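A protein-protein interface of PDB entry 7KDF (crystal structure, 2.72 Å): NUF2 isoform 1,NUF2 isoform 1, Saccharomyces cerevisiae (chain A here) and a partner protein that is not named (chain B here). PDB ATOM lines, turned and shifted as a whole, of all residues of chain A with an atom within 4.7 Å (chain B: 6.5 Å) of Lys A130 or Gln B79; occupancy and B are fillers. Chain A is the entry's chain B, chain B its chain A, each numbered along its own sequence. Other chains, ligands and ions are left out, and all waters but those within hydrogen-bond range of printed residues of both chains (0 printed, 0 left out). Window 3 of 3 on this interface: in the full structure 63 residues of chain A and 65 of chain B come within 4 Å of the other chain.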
ATOM      1  N   MET A 125       9.774   5.792  21.854  1.00  0.00           N
ATOM      2  CA  MET A 125       8.543   5.574  21.095  1.00  0.00           C
ATOM      3  C   MET A 125       8.756   4.758  19.831  1.00  0.00           C
ATOM      4  O   MET A 125       7.851   4.033  19.405  1.00  0.00           O
ATOM      5  CB  MET A 125       7.902   6.918  20.752  1.00  0.00           C
ATOM      6  CG  MET A 125       7.535   7.712  21.984  1.00  0.00           C
ATOM      7  SD  MET A 125       5.888   7.213  22.526  1.00  0.00           S
ATOM      8  CE  MET A 125       4.993   7.280  20.988  1.00  0.00           C
ATOM      9  N   THR A 126       9.935   4.857  19.218  1.00  0.00           N
ATOM     10  CA  THR A 126      10.201   4.061  18.026  1.00  0.00           C
ATOM     11  C   THR A 126      10.088   2.573  18.329  1.00  0.00           C
ATOM     12  O   THR A 126       9.524   1.807  17.537  1.00  0.00           O
ATOM     13  CB  THR A 126      11.586   4.393  17.475  1.00  0.00           C
ATOM     14  OG1 THR A 126      11.602   5.752  17.019  1.00  0.00           O
ATOM     15  CG2 THR A 126      11.944   3.462  16.322  1.00  0.00           C
ATOM     16  N   LEU A 128       8.187   1.068  20.265  1.00  0.00           N
ATOM     17  CA  LEU A 128       6.794   0.653  20.357  1.00  0.00           C
ATOM     18  C   LEU A 128       6.033   0.845  19.051  1.00  0.00           C
ATOM     19  O   LEU A 128       5.210  -0.002  18.685  1.00  0.00           O
ATOM     20  CB  LEU A 128       6.077   1.437  21.456  1.00  0.00           C
ATOM     21  CG  LEU A 128       6.210   1.047  22.916  1.00  0.00           C
ATOM     22  CD1 LEU A 128       5.514   2.100  23.755  1.00  0.00           C
ATOM     23  CD2 LEU A 128       5.608  -0.323  23.153  1.00  0.00           C
ATOM     24  N   TYR A 129       6.281   1.945  18.337  1.00  0.00           N
ATOM     25  CA  TYR A 129       5.364   2.381  17.299  1.00  0.00           C
ATOM     26  C   TYR A 129       5.933   2.369  15.899  1.00  0.00           C
ATOM     27  O   TYR A 129       5.186   2.611  14.943  1.00  0.00           O
ATOM     28  CB  TYR A 129       4.833   3.777  17.640  1.00  0.00           C
ATOM     29  CG  TYR A 129       3.986   3.625  18.852  1.00  0.00           C
ATOM     30  CD1 TYR A 129       2.785   2.941  18.773  1.00  0.00           C
ATOM     31  CD2 TYR A 129       4.429   4.039  20.090  1.00  0.00           C
ATOM     32  CE1 TYR A 129       2.013   2.741  19.875  1.00  0.00           C
ATOM     33  CE2 TYR A 129       3.672   3.833  21.208  1.00  0.00           C
ATOM     34  CZ  TYR A 129       2.455   3.183  21.095  1.00  0.00           C
ATOM     35  OH  TYR A 129       1.669   2.986  22.209  1.00  0.00           O
ATOM     36  N   LYS A 130       7.223   2.098  15.743  1.00  0.00           N
ATOM     37  CA  LYS A 130       7.784   1.727  14.449  1.00  0.00           C
ATOM     38  C   LYS A 130       8.981   0.830  14.710  1.00  0.00           C
ATOM     39  O   LYS A 130      10.134   1.204  14.469  1.00  0.00           O
ATOM     40  CB  LYS A 130       8.161   2.965  13.640  1.00  0.00           C
ATOM     41  CG  LYS A 130       8.545   2.630  12.216  1.00  0.00           C
ATOM     42  CD  LYS A 130       8.760   3.892  11.412  1.00  0.00           C
ATOM     43  CE  LYS A 130       9.103   3.574   9.960  1.00  0.00           C
ATOM     44  NZ  LYS A 130       9.335   4.821   9.162  1.00  0.00           N
ATOM     45  N   PRO A 131       8.740  -0.372  15.232  1.00  0.00           N
ATOM     46  CA  PRO A 131       9.848  -1.202  15.707  1.00  0.00           C
ATOM     47  C   PRO A 131      10.770  -1.609  14.571  1.00  0.00           C
ATOM     48  O   PRO A 131      10.353  -1.768  13.424  1.00  0.00           O
ATOM     49  CB  PRO A 131       9.147  -2.418  16.320  1.00  0.00           C
ATOM     50  CG  PRO A 131       7.708  -2.030  16.450  1.00  0.00           C
ATOM     51  CD  PRO A 131       7.448  -1.062  15.357  1.00  0.00           C
ATOM     52  N   GLU A 132      12.040  -1.782  14.909  1.00  0.00           N
ATOM     53  CA  GLU A 132      13.033  -2.244  13.957  1.00  0.00           C
ATOM     54  C   GLU A 132      13.762  -3.453  14.530  1.00  0.00           C
ATOM     55  O   GLU A 132      13.828  -3.645  15.749  1.00  0.00           O
ATOM     56  CB  GLU A 132      13.974  -1.090  13.569  1.00  0.00           C
ATOM     57  CG  GLU A 132      14.541  -0.292  14.724  1.00  0.00           C
ATOM     58  CD  GLU A 132      14.953   1.115  14.304  1.00  0.00           C
ATOM     59  OE1 GLU A 132      16.026   1.579  14.740  1.00  0.00           O
ATOM     60  OE2 GLU A 132      14.183   1.762  13.561  1.00  0.00           O
ATOM     61  N   TYR B  67      14.840   8.789  23.374  1.00  0.00           N
ATOM     62  CA  TYR B  67      14.832   8.874  21.921  1.00  0.00           C
ATOM     63  C   TYR B  67      16.190   9.312  21.386  1.00  0.00           C
ATOM     64  O   TYR B  67      16.826  10.226  21.919  1.00  0.00           O
ATOM     65  CB  TYR B  67      13.751   9.845  21.453  1.00  0.00           C
ATOM     66  CG  TYR B  67      13.534   9.840  19.953  1.00  0.00           C
ATOM     67  CD1 TYR B  67      12.585   9.008  19.374  1.00  0.00           C
ATOM     68  CD2 TYR B  67      14.272  10.670  19.119  1.00  0.00           C
ATOM     69  CE1 TYR B  67      12.381   8.999  18.007  1.00  0.00           C
ATOM     70  CE2 TYR B  67      14.069  10.670  17.747  1.00  0.00           C
ATOM     71  CZ  TYR B  67      13.123   9.834  17.200  1.00  0.00           C
ATOM     72  OH  TYR B  67      12.913   9.827  15.840  1.00  0.00           O
ATOM     73  N   ASN B  75      14.051  15.534   9.131  1.00  0.00           N
ATOM     74  CA  ASN B  75      13.500  14.379   8.430  1.00  0.00           C
ATOM     75  C   ASN B  75      12.715  13.435   9.330  1.00  0.00           C
ATOM     76  O   ASN B  75      12.138  12.469   8.820  1.00  0.00           O
ATOM     77  CB  ASN B  75      14.611  13.594   7.729  1.00  0.00           C
ATOM     78  CG  ASN B  75      15.541  14.481   6.941  1.00  0.00           C
ATOM     79  OD1 ASN B  75      16.718  14.607   7.269  1.00  0.00           O
ATOM     80  ND2 ASN B  75      15.014  15.112   5.895  1.00  0.00           N
ATOM     81  N   GLU B  76      12.676  13.671  10.641  1.00  0.00           N
ATOM     82  CA  GLU B  76      11.941  12.792  11.537  1.00  0.00           C
ATOM     83  C   GLU B  76      10.866  13.496  12.352  1.00  0.00           C
ATOM     84  O   GLU B  76      10.143  12.824  13.093  1.00  0.00           O
ATOM     85  CB  GLU B  76      12.904  12.067  12.486  1.00  0.00           C
ATOM     86  CG  GLU B  76      14.023  12.928  13.018  1.00  0.00           C
ATOM     87  CD  GLU B  76      15.037  12.125  13.803  1.00  0.00           C
ATOM     88  OE1 GLU B  76      14.887  10.889  13.879  1.00  0.00           O
ATOM     89  OE2 GLU B  76      15.991  12.727  14.339  1.00  0.00           O
ATOM     90  N   ILE B  77      10.722  14.818  12.225  1.00  0.00           N
ATOM     91  CA  ILE B  77       9.689  15.521  12.982  1.00  0.00           C
ATOM     92  C   ILE B  77       8.304  14.981  12.637  1.00  0.00           C
ATOM     93  O   ILE B  77       7.472  14.760  13.526  1.00  0.00           O
ATOM     94  CB  ILE B  77       9.790  17.040  12.744  1.00  0.00           C
ATOM     95  CG1 ILE B  77      10.936  17.630  13.570  1.00  0.00           C
ATOM     96  CG2 ILE B  77       8.470  17.738  13.066  1.00  0.00           C
ATOM     97  CD1 ILE B  77      11.191  19.092  13.296  1.00  0.00           C
ATOM     98  N   TYR B  78       8.037  14.747  11.351  1.00  0.00           N
ATOM     99  CA  TYR B  78       6.726  14.230  10.965  1.00  0.00           C
ATOM    100  C   TYR B  78       6.469  12.863  11.589  1.00  0.00           C
ATOM    101  O   TYR B  78       5.385  12.608  12.125  1.00  0.00           O
ATOM    102  CB  TYR B  78       6.604  14.156   9.440  1.00  0.00           C
ATOM    103  CG  TYR B  78       5.199  13.841   8.974  1.00  0.00           C
ATOM    104  CD1 TYR B  78       4.761  12.526   8.860  1.00  0.00           C
ATOM    105  CD2 TYR B  78       4.303  14.857   8.659  1.00  0.00           C
ATOM    106  CE1 TYR B  78       3.474  12.229   8.445  1.00  0.00           C
ATOM    107  CE2 TYR B  78       3.011  14.570   8.237  1.00  0.00           C
ATOM    108  CZ  TYR B  78       2.603  13.254   8.133  1.00  0.00           C
ATOM    109  OH  TYR B  78       1.323  12.953   7.718  1.00  0.00           O
ATOM    110  N   GLN B  79       7.458  11.968  11.532  1.00  0.00           N
ATOM    111  CA  GLN B  79       7.266  10.637  12.100  1.00  0.00           C
ATOM    112  C   GLN B  79       7.080  10.711  13.610  1.00  0.00           C
ATOM    113  O   GLN B  79       6.267   9.974  14.181  1.00  0.00           O
ATOM    114  CB  GLN B  79       8.442   9.728  11.743  1.00  0.00           C
ATOM    115  CG  GLN B  79       8.270   8.294  12.227  1.00  0.00           C
ATOM    116  CD  GLN B  79       7.269   7.517  11.394  1.00  0.00           C
ATOM    117  OE1 GLN B  79       7.285   7.581  10.165  1.00  0.00           O
ATOM    118  NE2 GLN B  79       6.379   6.791  12.062  1.00  0.00           N
ATOM    119  N   ILE B  80       7.823  11.602  14.269  1.00  0.00           N
ATOM    120  CA  ILE B  80       7.680  11.778  15.711  1.00  0.00           C
ATOM    121  C   ILE B  80       6.259  12.206  16.052  1.00  0.00           C
ATOM    122  O   ILE B  80       5.635  11.673  16.979  1.00  0.00           O
ATOM    123  CB  ILE B  80       8.713  12.795  16.229  1.00  0.00           C
ATOM    124  CG1 ILE B  80      10.128  12.228  16.110  1.00  0.00           C
ATOM    125  CG2 ILE B  80       8.405  13.180  17.663  1.00  0.00           C
ATOM    126  CD1 ILE B  80      11.204  13.192  16.556  1.00  0.00           C
ATOM    127  N   LEU B  81       5.720  13.167  15.300  1.00  0.00           N
ATOM    128  CA  LEU B  81       4.355  13.611  15.561  1.00  0.00           C
ATOM    129  C   LEU B  81       3.340  12.523  15.242  1.00  0.00           C
ATOM    130  O   LEU B  81       2.308  12.430  15.914  1.00  0.00           O
ATOM    131  CB  LEU B  81       4.048  14.879  14.769  1.00  0.00           C
ATOM    132  CG  LEU B  81       4.944  16.068  15.117  1.00  0.00           C
ATOM    133  CD1 LEU B  81       4.979  17.075  13.973  1.00  0.00           C
ATOM    134  CD2 LEU B  81       4.481  16.719  16.410  1.00  0.00           C
ATOM    135  N   LYS B  82       3.607  11.701  14.225  1.00  0.00           N
ATOM    136  CA  LYS B  82       2.707  10.594  13.916  1.00  0.00           C
ATOM    137  C   LYS B  82       2.645   9.608  15.077  1.00  0.00           C
ATOM    138  O   LYS B  82       1.561   9.169  15.477  1.00  0.00           O
ATOM    139  CB  LYS B  82       3.153   9.892  12.633  1.00  0.00           C
ATOM    140  CG  LYS B  82       2.143   8.877  12.102  1.00  0.00           C
ATOM    141  CD  LYS B  82       2.359   8.599  10.619  1.00  0.00           C
ATOM    142  CE  LYS B  82       1.496   7.444  10.128  1.00  0.00           C
ATOM    143  NZ  LYS B  82       1.871   6.141  10.751  1.00  0.00           N
ATOM    144  N   ASN B  83       3.807   9.255  15.635  1.00  0.00           N
ATOM    145  CA  ASN B  83       3.842   8.381  16.803  1.00  0.00           C
ATOM    146  C   ASN B  83       3.209   9.052  18.012  1.00  0.00           C
ATOM    147  O   ASN B  83       2.493   8.405  18.785  1.00  0.00           O
ATOM    148  CB  ASN B  83       5.279   7.980  17.116  1.00  0.00           C
ATOM    149  CG  ASN B  83       5.951   7.295  15.957  1.00  0.00           C
ATOM    150  OD1 ASN B  83       5.288   6.787  15.049  1.00  0.00           O
ATOM    151  ND2 ASN B  83       7.278   7.279  15.972  1.00  0.00           N
ATOM    152  N   LEU B  84       3.464  10.351  18.193  1.00  0.00           N
ATOM    153  CA  LEU B  84       2.815  11.103  19.260  1.00  0.00           C
ATOM    154  C   LEU B  84       1.309  11.167  19.063  1.00  0.00           C
ATOM    155  O   LEU B  84       0.580  11.514  20.000  1.00  0.00           O
ATOM    156  CB  LEU B  84       3.389  12.518  19.326  1.00  0.00           C
ATOM    157  CG  LEU B  84       4.724  12.663  20.050  1.00  0.00           C
ATOM    158  CD1 LEU B  84       5.270  14.062  19.863  1.00  0.00           C
ATOM    159  CD2 LEU B  84       4.574  12.328  21.525  1.00  0.00           C
ATOM    160  N   LEU B  89      -2.032  16.534  12.651  1.00  0.00           N
ATOM    161  CA  LEU B  89      -0.974  16.093  11.747  1.00  0.00           C
ATOM    162  C   LEU B  89      -1.325  16.375  10.290  1.00  0.00           C
ATOM    163  O   LEU B  89      -0.482  16.867   9.528  1.00  0.00           O
ATOM    164  CB  LEU B  89      -0.699  14.603  11.953  1.00  0.00           C
ATOM    165  CG  LEU B  89       0.498  14.003  11.208  1.00  0.00           C
ATOM    166  CD1 LEU B  89       1.797  14.685  11.614  1.00  0.00           C
ATOM    167  CD2 LEU B  89       0.581  12.507  11.461  1.00  0.00           C
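OD1 of Asn B83 lies within hydrogen-bond range of NE2 of Gln B79 (3.2 Å). The side-chain hydroxyl (OH) of Tyr B67 sits at hydrogen-bond distance from the side-chain carboxylate (OE1) of Glu B76.
Met A125 touches Asn B83 (CE to O, 3.5 Å). Thr A126 touches Tyr B67 (OG1 to CE1, 3.5 Å). CB of Tyr A129 touches OD1 of Asn B83, at 3.998 Å. Lys A130 touches Gln B79 (NZ to OE1, 3.6 Å).
Lys A130 touches just one residue of chain B: Gln B79. Of chain A, only Lys A130 comes within 4 Å of Gln B79. Of the printed residues of chain A, Tyr B67 touches Thr A126. Of the printed residues of chain B, Tyr A129 touches Asn B83. Leu B89 touches none of the printed residues of chain A. The nearest printed residue of chain A that does not touch Tyr B67 is Met A125 (4.9 Å).
Hydrophobic or aromatic side chains of chain B within 4 Å of the printed part of chain A: Tyr B67. Printed residues of chain A that touch a printed residue of chain B: Met A125, Thr A126, Tyr A129 and Lys A130. Hydrophobic or aromatic side chains of chain A within 4 Å of the printed part of chain B: Met A125 and Tyr A129. Among the printed residues, 4 pairs touch across the chains. Among the printed residues, no Asp or Glu carboxylate lies within 4 Å of a Lys or Arg side-chain nitrogen of the other chain.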
